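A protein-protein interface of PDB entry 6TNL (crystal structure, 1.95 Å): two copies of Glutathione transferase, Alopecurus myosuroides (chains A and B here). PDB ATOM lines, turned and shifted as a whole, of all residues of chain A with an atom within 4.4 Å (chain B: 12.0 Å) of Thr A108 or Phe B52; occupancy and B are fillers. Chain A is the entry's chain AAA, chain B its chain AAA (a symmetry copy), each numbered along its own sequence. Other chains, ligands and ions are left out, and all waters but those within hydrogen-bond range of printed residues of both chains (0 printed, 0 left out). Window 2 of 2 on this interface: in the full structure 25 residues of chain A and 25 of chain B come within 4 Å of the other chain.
Hydrophobic or aromatic side chains of chain B within 4 Å of the printed part of chain A: Pro B51, Phe B52 and Trp B66.
Of the 12 printed residues of chain A, 4 touch a printed residue of chain B.
Position printed for both chains: 107.
Of the 7 pairs that touch across the chains among the printed residues, none has its exchanged pair printed and touching as well.
Of the printed residues of chain B, Val A104 touches Phe B52, Trp B66 and Glu B67.
No residue of chain B comes within 4 Å of Asp A105.
Thr A108 touches just one residue of chain B: Phe B52.
No residue of chain B comes within 4 Å of Asn A110.
No residue of chain B comes within 4 Å of Pro A111.
No residue of chain B comes within 4 Å of Ala A112.
Val A146 touches none of the printed residues of chain B.
Val A149 touches just these residues of chain B: Pro B51 (3.8 Å) and Phe B52 (3.2 Å).
Tyr A150 touches none of the printed residues of chain B.
Of the printed residues of chain A, Pro B51 touches Val A149 (3.8 Å).
Of chain A, only Val A104 (3.5 Å), Thr A108 (3.9 Å) and Val A149 (3.2 Å) come within 4 Å of Phe B52.
Printed residues of chain A within 4 Å of Trp B66: Val A104.
Printed residues of chain A within 4 Å of Glu B67: Val A104 (3.99 Å) and His A107 (3.1 Å).
His B107 touches none of the printed residues of chain A.
The nearest residue of chain B that does not touch Thr A108 is Gln B54 (4.3 Å).
The nearest printed residue of chain A that does not touch Phe B52 is Tyr A150 (4.2 Å).
Among the printed residues, merely in contact across the chains: Val A104 with Phe B52 (3.5 Å), Val A104 with Trp B66 (3.8 Å), Val A104 with Glu B67 (3.99 Å), His A107 with Glu B67 (3.1 Å), Thr A108 with Phe B52 (3.9 Å), Val A149 with Pro B51 (3.8 Å) and Val A149 with Phe B52 (3.2 Å).
The side-chain amide nitrogen of Gln B54 sits at hydrogen-bond distance from the side-chain carboxylate of Glu B67, at 3.4 Å.
The backbone NH of Tyr A109 is in hydrogen-bond range of the backbone carbonyl oxygen of Val A104 (3.1 Å).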
ATOM      1  N   VAL A 104     -24.159 -31.868  25.450  1.00  0.00           N
ATOM      2  CA  VAL A 104     -23.902 -33.028  24.548  1.00  0.00           C
ATOM      3  C   VAL A 104     -25.140 -33.955  24.619  1.00  0.00           C
ATOM      4  O   VAL A 104     -25.626 -34.359  23.558  1.00  0.00           O
ATOM      5  CB  VAL A 104     -22.584 -33.761  24.878  1.00  0.00           C
ATOM      6  CG1 VAL A 104     -22.441 -35.050  24.083  1.00  0.00           C
ATOM      7  CG2 VAL A 104     -21.402 -32.855  24.577  1.00  0.00           C
ATOM      8  N   ASP A 105     -25.644 -34.208  25.812  1.00  0.00           N
ATOM      9  CA  ASP A 105     -26.857 -35.024  26.034  1.00  0.00           C
ATOM     10  C   ASP A 105     -28.050 -34.429  25.246  1.00  0.00           C
ATOM     11  O   ASP A 105     -28.720 -35.180  24.501  1.00  0.00           O
ATOM     12  CB  ASP A 105     -27.215 -35.099  27.499  1.00  0.00           C
ATOM     13  CG  ASP A 105     -28.446 -35.962  27.695  1.00  0.00           C
ATOM     14  OD1 ASP A 105     -28.464 -37.071  27.121  1.00  0.00           O
ATOM     15  OD2 ASP A 105     -29.447 -35.412  28.136  1.00  0.00           O
ATOM     16  N   ALA A 106     -28.297 -33.119  25.389  1.00  0.00           N
ATOM     17  CA  ALA A 106     -29.438 -32.439  24.720  1.00  0.00           C
ATOM     18  C   ALA A 106     -29.253 -32.439  23.209  1.00  0.00           C
ATOM     19  O   ALA A 106     -30.263 -32.639  22.527  1.00  0.00           O
ATOM     20  CB  ALA A 106     -29.627 -31.030  25.256  1.00  0.00           C
ATOM     21  N   HIS A 107     -28.062 -32.100  22.682  1.00  0.00           N
ATOM     22  CA  HIS A 107     -27.846 -31.763  21.261  1.00  0.00           C
ATOM     23  C   HIS A 107     -27.387 -32.951  20.420  1.00  0.00           C
ATOM     24  O   HIS A 107     -27.565 -32.875  19.235  1.00  0.00           O
ATOM     25  CB  HIS A 107     -26.826 -30.621  21.104  1.00  0.00           C
ATOM     26  CG  HIS A 107     -27.271 -29.361  21.772  1.00  0.00           C
ATOM     27  ND1 HIS A 107     -28.609 -28.987  21.853  1.00  0.00           N
ATOM     28  CD2 HIS A 107     -26.570 -28.374  22.371  1.00  0.00           C
ATOM     29  CE1 HIS A 107     -28.706 -27.815  22.465  1.00  0.00           C
ATOM     30  NE2 HIS A 107     -27.470 -27.414  22.785  1.00  0.00           N
ATOM     31  N   THR A 108     -26.819 -34.000  21.006  1.00  0.00           N
ATOM     32  CA  THR A 108     -26.101 -35.047  20.247  1.00  0.00           C
ATOM     33  C   THR A 108     -26.629 -36.419  20.662  1.00  0.00           C
ATOM     34  O   THR A 108     -27.046 -37.133  19.817  1.00  0.00           O
ATOM     35  CB  THR A 108     -24.590 -34.913  20.470  1.00  0.00           C
ATOM     36  OG1 THR A 108     -24.260 -33.611  20.009  1.00  0.00           O
ATOM     37  CG2 THR A 108     -23.774 -35.973  19.755  1.00  0.00           C
ATOM     38  N   TYR A 109     -26.610 -36.752  21.937  1.00  0.00           N
ATOM     39  CA  TYR A 109     -26.936 -38.094  22.439  1.00  0.00           C
ATOM     40  C   TYR A 109     -28.442 -38.364  22.376  1.00  0.00           C
ATOM     41  O   TYR A 109     -28.835 -39.335  21.729  1.00  0.00           O
ATOM     42  CB  TYR A 109     -26.382 -38.248  23.846  1.00  0.00           C
ATOM     43  CG  TYR A 109     -26.549 -39.617  24.454  1.00  0.00           C
ATOM     44  CD1 TYR A 109     -25.559 -40.571  24.331  1.00  0.00           C
ATOM     45  CD2 TYR A 109     -27.659 -39.916  25.235  1.00  0.00           C
ATOM     46  CE1 TYR A 109     -25.650 -41.795  24.966  1.00  0.00           C
ATOM     47  CE2 TYR A 109     -27.769 -41.150  25.872  1.00  0.00           C
ATOM     48  CZ  TYR A 109     -26.761 -42.087  25.734  1.00  0.00           C
ATOM     49  OH  TYR A 109     -26.848 -43.286  26.331  1.00  0.00           O
ATOM     50  N   ASN A 110     -29.251 -37.595  23.083  1.00  0.00           N
ATOM     51  CA  ASN A 110     -30.717 -37.824  23.133  1.00  0.00           C
ATOM     52  C   ASN A 110     -31.285 -37.850  21.716  1.00  0.00           C
ATOM     53  O   ASN A 110     -32.091 -38.724  21.399  1.00  0.00           O
ATOM     54  CB  ASN A 110     -31.474 -36.838  24.012  1.00  0.00           C
ATOM     55  CG  ASN A 110     -31.376 -37.088  25.495  1.00  0.00           C
ATOM     56  OD1 ASN A 110     -30.813 -38.072  26.010  1.00  0.00           O
ATOM     57  ND2 ASN A 110     -31.946 -36.170  26.240  1.00  0.00           N
ATOM     58  N   PRO A 111     -30.922 -36.945  20.789  1.00  0.00           N
ATOM     59  CA  PRO A 111     -31.375 -37.080  19.409  1.00  0.00           C
ATOM     60  C   PRO A 111     -30.894 -38.313  18.620  1.00  0.00           C
ATOM     61  O   PRO A 111     -31.510 -38.676  17.646  1.00  0.00           O
ATOM     62  CB  PRO A 111     -30.901 -35.805  18.674  1.00  0.00           C
ATOM     63  CG  PRO A 111     -30.111 -35.016  19.685  1.00  0.00           C
ATOM     64  CD  PRO A 111     -30.282 -35.649  21.049  1.00  0.00           C
ATOM     65  N   ALA A 112     -29.758 -38.881  18.957  1.00  0.00           N
ATOM     66  CA  ALA A 112     -29.290 -40.125  18.310  1.00  0.00           C
ATOM     67  C   ALA A 112     -30.134 -41.310  18.821  1.00  0.00           C
ATOM     68  O   ALA A 112     -30.358 -42.218  18.022  1.00  0.00           O
ATOM     69  CB  ALA A 112     -27.820 -40.338  18.578  1.00  0.00           C
ATOM     70  N   VAL A 146     -21.336 -41.632  18.004  1.00  0.00           N
ATOM     71  CA  VAL A 146     -21.450 -40.916  19.296  1.00  0.00           C
ATOM     72  C   VAL A 146     -20.855 -41.802  20.411  1.00  0.00           C
ATOM     73  O   VAL A 146     -20.138 -41.255  21.246  1.00  0.00           O
ATOM     74  CB  VAL A 146     -22.899 -40.541  19.590  1.00  0.00           C
ATOM     75  CG1 VAL A 146     -23.057 -40.051  21.023  1.00  0.00           C
ATOM     76  CG2 VAL A 146     -23.455 -39.551  18.561  1.00  0.00           C
ATOM     77  N   VAL A 149     -17.132 -41.755  20.895  1.00  0.00           N
ATOM     78  CA  VAL A 149     -16.677 -40.548  21.628  1.00  0.00           C
ATOM     79  C   VAL A 149     -16.905 -40.768  23.122  1.00  0.00           C
ATOM     80  O   VAL A 149     -16.018 -40.408  23.941  1.00  0.00           O
ATOM     81  CB  VAL A 149     -17.406 -39.305  21.077  1.00  0.00           C
ATOM     82  CG1 VAL A 149     -17.300 -38.135  22.034  1.00  0.00           C
ATOM     83  CG2 VAL A 149     -16.912 -38.945  19.694  1.00  0.00           C
ATOM     84  N   TYR A 150     -18.060 -41.312  23.493  1.00  0.00           N
ATOM     85  CA  TYR A 150     -18.373 -41.539  24.920  1.00  0.00           C
ATOM     86  C   TYR A 150     -17.372 -42.554  25.483  1.00  0.00           C
ATOM     87  O   TYR A 150     -16.971 -42.401  26.667  1.00  0.00           O
ATOM     88  CB  TYR A 150     -19.826 -41.972  25.097  1.00  0.00           C
ATOM     89  CG  TYR A 150     -20.823 -40.850  25.221  1.00  0.00           C
ATOM     90  CD1 TYR A 150     -21.070 -39.973  24.191  1.00  0.00           C
ATOM     91  CD2 TYR A 150     -21.553 -40.668  26.383  1.00  0.00           C
ATOM     92  CE1 TYR A 150     -21.968 -38.924  24.324  1.00  0.00           C
ATOM     93  CE2 TYR A 150     -22.479 -39.651  26.529  1.00  0.00           C
ATOM     94  CZ  TYR A 150     -22.681 -38.765  25.493  1.00  0.00           C
ATOM     95  OH  TYR A 150     -23.620 -37.786  25.603  1.00  0.00           O
ATOM     96  N   PHE B   7     -13.107 -19.741  18.576  1.00  0.00           N
ATOM     97  CA  PHE B   7     -12.837 -20.238  17.213  1.00  0.00           C
ATOM     98  C   PHE B   7     -14.186 -20.422  16.509  1.00  0.00           C
ATOM     99  O   PHE B   7     -15.015 -21.201  16.963  1.00  0.00           O
ATOM    100  CB  PHE B   7     -12.065 -21.545  17.237  1.00  0.00           C
ATOM    101  CG  PHE B   7     -10.704 -21.472  17.883  1.00  0.00           C
ATOM    102  CD1 PHE B   7     -10.528 -21.695  19.242  1.00  0.00           C
ATOM    103  CD2 PHE B   7      -9.581 -21.250  17.117  1.00  0.00           C
ATOM    104  CE1 PHE B   7      -9.261 -21.662  19.833  1.00  0.00           C
ATOM    105  CE2 PHE B   7      -8.313 -21.205  17.703  1.00  0.00           C
ATOM    106  CZ  PHE B   7      -8.161 -21.407  19.057  1.00  0.00           C
ATOM    107  N   ASN B  14     -24.249 -18.825  17.361  1.00  0.00           N
ATOM    108  CA  ASN B  14     -23.591 -19.502  18.503  1.00  0.00           C
ATOM    109  C   ASN B  14     -22.286 -18.790  18.908  1.00  0.00           C
ATOM    110  O   ASN B  14     -21.976 -18.791  20.117  1.00  0.00           O
ATOM    111  CB  ASN B  14     -23.386 -20.979  18.204  1.00  0.00           C
ATOM    112  CG  ASN B  14     -24.663 -21.735  18.483  1.00  0.00           C
ATOM    113  OD1 ASN B  14     -25.466 -21.330  19.320  1.00  0.00           O
ATOM    114  ND2 ASN B  14     -24.853 -22.821  17.794  1.00  0.00           N
ATOM    115  N   ILE B  34     -11.702 -20.516  11.889  1.00  0.00           N
ATOM    116  CA  ILE B  34     -11.057 -21.821  11.587  1.00  0.00           C
ATOM    117  C   ILE B  34     -11.844 -22.439  10.458  1.00  0.00           C
ATOM    118  O   ILE B  34     -13.027 -22.206  10.359  1.00  0.00           O
ATOM    119  CB  ILE B  34     -10.922 -22.786  12.772  1.00  0.00           C
ATOM    120  CG1 ILE B  34     -12.088 -22.627  13.741  1.00  0.00           C
ATOM    121  CG2 ILE B  34      -9.536 -22.640  13.401  1.00  0.00           C
ATOM    122  CD1 ILE B  34     -13.405 -23.095  13.215  1.00  0.00           C
ATOM    123  N   PHE B  36     -12.466 -26.283   8.746  1.00  0.00           N
ATOM    124  CA  PHE B  36     -12.320 -27.746   8.944  1.00  0.00           C
ATOM    125  C   PHE B  36     -11.160 -28.364   8.134  1.00  0.00           C
ATOM    126  O   PHE B  36     -10.819 -29.521   8.492  1.00  0.00           O
ATOM    127  CB  PHE B  36     -13.643 -28.433   8.626  1.00  0.00           C
ATOM    128  CG  PHE B  36     -14.683 -28.168   9.679  1.00  0.00           C
ATOM    129  CD1 PHE B  36     -14.381 -28.302  11.024  1.00  0.00           C
ATOM    130  CD2 PHE B  36     -15.951 -27.745   9.331  1.00  0.00           C
ATOM    131  CE1 PHE B  36     -15.353 -28.095  11.994  1.00  0.00           C
ATOM    132  CE2 PHE B  36     -16.915 -27.512  10.301  1.00  0.00           C
ATOM    133  CZ  PHE B  36     -16.615 -27.692  11.627  1.00  0.00           C
ATOM    134  N   ASN B  50     -11.881 -31.608  21.551  1.00  0.00           N
ATOM    135  CA  ASN B  50     -13.124 -31.243  20.823  1.00  0.00           C
ATOM    136  C   ASN B  50     -13.591 -32.458  20.033  1.00  0.00           C
ATOM    137  O   ASN B  50     -13.492 -32.467  18.817  1.00  0.00           O
ATOM    138  CB  ASN B  50     -12.837 -30.020  19.958  1.00  0.00           C
ATOM    139  CG  ASN B  50     -14.044 -29.473  19.229  1.00  0.00           C
ATOM    140  OD1 ASN B  50     -13.942 -28.570  18.389  1.00  0.00           O
ATOM    141  ND2 ASN B  50     -15.185 -30.088  19.490  1.00  0.00           N
ATOM    142  N   PRO B  51     -14.057 -33.554  20.694  1.00  0.00           N
ATOM    143  CA  PRO B  51     -14.213 -34.853  20.032  1.00  0.00           C
ATOM    144  C   PRO B  51     -15.319 -34.932  18.962  1.00  0.00           C
ATOM    145  O   PRO B  51     -15.157 -35.699  18.066  1.00  0.00           O
ATOM    146  CB  PRO B  51     -14.411 -35.855  21.193  1.00  0.00           C
ATOM    147  CG  PRO B  51     -14.899 -35.018  22.375  1.00  0.00           C
ATOM    148  CD  PRO B  51     -14.356 -33.632  22.132  1.00  0.00           C
ATOM    149  N   PHE B  52     -16.388 -34.140  19.032  1.00  0.00           N
ATOM    150  CA  PHE B  52     -17.411 -34.084  17.951  1.00  0.00           C
ATOM    151  C   PHE B  52     -17.072 -32.981  16.945  1.00  0.00           C
ATOM    152  O   PHE B  52     -18.050 -32.605  16.244  1.00  0.00           O
ATOM    153  CB  PHE B  52     -18.817 -33.776  18.485  1.00  0.00           C
ATOM    154  CG  PHE B  52     -19.327 -34.799  19.469  1.00  0.00           C
ATOM    155  CD1 PHE B  52     -19.591 -36.104  19.067  1.00  0.00           C
ATOM    156  CD2 PHE B  52     -19.407 -34.501  20.820  1.00  0.00           C
ATOM    157  CE1 PHE B  52     -19.986 -37.060  19.989  1.00  0.00           C
ATOM    158  CE2 PHE B  52     -19.833 -35.448  21.738  1.00  0.00           C
ATOM    159  CZ  PHE B  52     -20.117 -36.724  21.318  1.00  0.00           C
ATOM    160  N   GLY B  53     -15.840 -32.407  16.980  1.00  0.00           N
ATOM    161  CA  GLY B  53     -15.361 -31.292  16.132  1.00  0.00           C
ATOM    162  C   GLY B  53     -16.388 -30.190  15.910  1.00  0.00           C
ATOM    163  O   GLY B  53     -16.695 -29.876  14.735  1.00  0.00           O
ATOM    164  N   GLN B  54     -16.869 -29.558  16.993  1.00  0.00           N
ATOM    165  CA  GLN B  54     -17.911 -28.505  16.924  1.00  0.00           C
ATOM    166  C   GLN B  54     -17.271 -27.111  16.978  1.00  0.00           C
ATOM    167  O   GLN B  54     -16.101 -26.974  17.411  1.00  0.00           O
ATOM    168  CB  GLN B  54     -18.916 -28.634  18.065  1.00  0.00           C
ATOM    169  CG  GLN B  54     -19.937 -29.729  17.835  1.00  0.00           C
ATOM    170  CD  GLN B  54     -20.803 -29.909  19.058  1.00  0.00           C
ATOM    171  OE1 GLN B  54     -20.834 -30.971  19.676  1.00  0.00           O
ATOM    172  NE2 GLN B  54     -21.476 -28.837  19.438  1.00  0.00           N
ATOM    173  N   ILE B  55     -18.034 -26.149  16.490  1.00  0.00           N
ATOM    174  CA  ILE B  55     -17.732 -24.701  16.417  1.00  0.00           C
ATOM    175  C   ILE B  55     -18.936 -24.022  17.045  1.00  0.00           C
ATOM    176  O   ILE B  55     -20.025 -24.455  16.772  1.00  0.00           O
ATOM    177  CB  ILE B  55     -17.458 -24.310  14.944  1.00  0.00           C
ATOM    178  CG1 ILE B  55     -16.055 -24.799  14.585  1.00  0.00           C
ATOM    179  CG2 ILE B  55     -17.566 -22.826  14.713  1.00  0.00           C
ATOM    180  CD1 ILE B  55     -16.011 -25.717  13.456  1.00  0.00           C
ATOM    181  N   PRO B  56     -18.810 -23.048  17.959  1.00  0.00           N
ATOM    182  CA  PRO B  56     -17.527 -22.484  18.391  1.00  0.00           C
ATOM    183  C   PRO B  56     -16.742 -23.418  19.330  1.00  0.00           C
ATOM    184  O   PRO B  56     -17.343 -24.306  19.981  1.00  0.00           O
ATOM    185  CB  PRO B  56     -17.906 -21.244  19.189  1.00  0.00           C
ATOM    186  CG  PRO B  56     -19.275 -21.617  19.733  1.00  0.00           C
ATOM    187  CD  PRO B  56     -19.945 -22.476  18.673  1.00  0.00           C
ATOM    188  N   ALA B  57     -15.422 -23.321  19.265  1.00  0.00           N
ATOM    189  CA  ALA B  57     -14.528 -23.927  20.287  1.00  0.00           C
ATOM    190  C   ALA B  57     -13.916 -22.756  21.036  1.00  0.00           C
ATOM    191  O   ALA B  57     -14.039 -21.615  20.564  1.00  0.00           O
ATOM    192  CB  ALA B  57     -13.496 -24.821  19.651  1.00  0.00           C
ATOM    193  N   PHE B  58     -13.348 -23.002  22.207  1.00  0.00           N
ATOM    194  CA  PHE B  58     -12.956 -21.911  23.135  1.00  0.00           C
ATOM    195  C   PHE B  58     -11.710 -22.402  23.860  1.00  0.00           C
ATOM    196  O   PHE B  58     -11.774 -23.563  24.306  1.00  0.00           O
ATOM    197  CB  PHE B  58     -14.115 -21.576  24.079  1.00  0.00           C
ATOM    198  CG  PHE B  58     -13.776 -20.621  25.190  1.00  0.00           C
ATOM    199  CD1 PHE B  58     -13.817 -19.252  24.997  1.00  0.00           C
ATOM    200  CD2 PHE B  58     -13.420 -21.094  26.442  1.00  0.00           C
ATOM    201  CE1 PHE B  58     -13.553 -18.372  26.041  1.00  0.00           C
ATOM    202  CE2 PHE B  58     -13.123 -20.215  27.478  1.00  0.00           C
ATOM    203  CZ  PHE B  58     -13.189 -18.857  27.276  1.00  0.00           C
ATOM    204  N   LEU B  64      -9.800 -26.417  26.847  1.00  0.00           N
ATOM    205  CA  LEU B  64     -10.534 -26.349  25.560  1.00  0.00           C
ATOM    206  C   LEU B  64     -11.991 -26.727  25.810  1.00  0.00           C
ATOM    207  O   LEU B  64     -12.237 -27.785  26.308  1.00  0.00           O
ATOM    208  CB  LEU B  64      -9.881 -27.201  24.500  1.00  0.00           C
ATOM    209  N   LEU B  65     -12.922 -25.844  25.470  1.00  0.00           N
ATOM    210  CA  LEU B  65     -14.374 -26.050  25.667  1.00  0.00           C
ATOM    211  C   LEU B  65     -15.076 -25.984  24.304  1.00  0.00           C
ATOM    212  O   LEU B  65     -14.549 -25.378  23.385  1.00  0.00           O
ATOM    213  CB  LEU B  65     -14.973 -24.979  26.583  1.00  0.00           C
ATOM    214  CG  LEU B  65     -14.526 -24.977  28.048  1.00  0.00           C
ATOM    215  CD1 LEU B  65     -15.270 -23.859  28.810  1.00  0.00           C
ATOM    216  CD2 LEU B  65     -14.746 -26.311  28.701  1.00  0.00           C
ATOM    217  N   TRP B  66     -16.270 -26.536  24.238  1.00  0.00           N
ATOM    218  CA  TRP B  66     -17.218 -26.462  23.094  1.00  0.00           C
ATOM    219  C   TRP B  66     -18.616 -26.470  23.701  1.00  0.00           C
ATOM    220  O   TRP B  66     -18.711 -26.650  24.911  1.00  0.00           O
ATOM    221  CB  TRP B  66     -16.982 -27.599  22.098  1.00  0.00           C
ATOM    222  CG  TRP B  66     -17.496 -28.941  22.541  1.00  0.00           C
ATOM    223  CD1 TRP B  66     -18.715 -29.516  22.265  1.00  0.00           C
ATOM    224  CD2 TRP B  66     -16.791 -29.897  23.345  1.00  0.00           C
ATOM    225  NE1 TRP B  66     -18.803 -30.755  22.832  1.00  0.00           N
ATOM    226  CE2 TRP B  66     -17.640 -31.028  23.483  1.00  0.00           C
ATOM    227  CE3 TRP B  66     -15.514 -29.931  23.912  1.00  0.00           C
ATOM    228  CZ2 TRP B  66     -17.281 -32.165  24.209  1.00  0.00           C
ATOM    229  CZ3 TRP B  66     -15.155 -31.052  24.630  1.00  0.00           C
ATOM    230  CH2 TRP B  66     -16.021 -32.156  24.770  1.00  0.00           C
ATOM    231  N   GLU B  67     -19.651 -26.237  22.887  1.00  0.00           N
ATOM    232  CA  GLU B  67     -21.050 -26.040  23.304  1.00  0.00           C
ATOM    233  C   GLU B  67     -21.147 -24.584  23.745  1.00  0.00           C
ATOM    234  O   GLU B  67     -20.696 -24.213  24.847  1.00  0.00           O
ATOM    235  CB  GLU B  67     -21.568 -27.056  24.328  1.00  0.00           C
ATOM    236  CG  GLU B  67     -21.740 -28.448  23.797  1.00  0.00           C
ATOM    237  CD  GLU B  67     -22.931 -28.523  22.867  1.00  0.00           C
ATOM    238  OE1 GLU B  67     -23.613 -27.541  22.711  1.00  0.00           O
ATOM    239  OE2 GLU B  67     -23.172 -29.570  22.347  1.00  0.00           O
ATOM    240  N   SER B  68     -21.795 -23.805  22.893  1.00  0.00           N
ATOM    241  CA  SER B  68     -21.920 -22.349  23.002  1.00  0.00           C
ATOM    242  C   SER B  68     -22.412 -21.986  24.404  1.00  0.00           C
ATOM    243  O   SER B  68     -21.916 -21.060  24.989  1.00  0.00           O
ATOM    244  CB  SER B  68     -22.891 -21.889  21.933  1.00  0.00           C
ATOM    245  OG  SER B  68     -22.970 -20.490  21.959  1.00  0.00           O
ATOM    246  N   ARG B  69     -23.461 -22.653  24.871  1.00  0.00           N
ATOM    247  CA  ARG B  69     -24.067 -22.334  26.179  1.00  0.00           C
ATOM    248  C   ARG B  69     -23.066 -22.662  27.311  1.00  0.00           C
ATOM    249  O   ARG B  69     -23.035 -21.899  28.251  1.00  0.00           O
ATOM    250  CB  ARG B  69     -25.383 -23.093  26.365  1.00  0.00           C
ATOM    251  CG  ARG B  69     -26.582 -22.332  25.819  1.00  0.00           C
ATOM    252  CD  ARG B  69     -27.937 -22.995  26.042  1.00  0.00           C
ATOM    253  NE  ARG B  69     -28.347 -23.678  24.817  1.00  0.00           N
ATOM    254  CZ  ARG B  69     -28.939 -23.117  23.764  1.00  0.00           C
ATOM    255  NH1 ARG B  69     -29.287 -21.849  23.799  1.00  0.00           N
ATOM    256  NH2 ARG B  69     -29.313 -23.839  22.728  1.00  0.00           N
ATOM    257  N   ALA B  70     -22.354 -23.767  27.234  1.00  0.00           N
ATOM    258  CA  ALA B  70     -21.376 -24.132  28.290  1.00  0.00           C
ATOM    259  C   ALA B  70     -20.230 -23.102  28.266  1.00  0.00           C
ATOM    260  O   ALA B  70     -19.779 -22.627  29.390  1.00  0.00           O
ATOM    261  CB  ALA B  70     -20.890 -25.540  28.112  1.00  0.00           C
ATOM    262  N   HIS B 107     -36.052 -23.493  23.396  1.00  0.00           N
ATOM    263  CA  HIS B 107     -37.110 -24.466  23.053  1.00  0.00           C
ATOM    264  C   HIS B 107     -38.306 -23.833  22.346  1.00  0.00           C
ATOM    265  O   HIS B 107     -39.001 -24.567  21.699  1.00  0.00           O
ATOM    266  CB  HIS B 107     -37.610 -25.216  24.300  1.00  0.00           C
ATOM    267  CG  HIS B 107     -36.527 -25.994  24.972  1.00  0.00           C
ATOM    268  ND1 HIS B 107     -35.485 -26.591  24.268  1.00  0.00           N
ATOM    269  CD2 HIS B 107     -36.323 -26.299  26.271  1.00  0.00           C
ATOM    270  CE1 HIS B 107     -34.694 -27.240  25.112  1.00  0.00           C
ATOM    271  NE2 HIS B 107     -35.191 -27.084  26.345  1.00  0.00           N
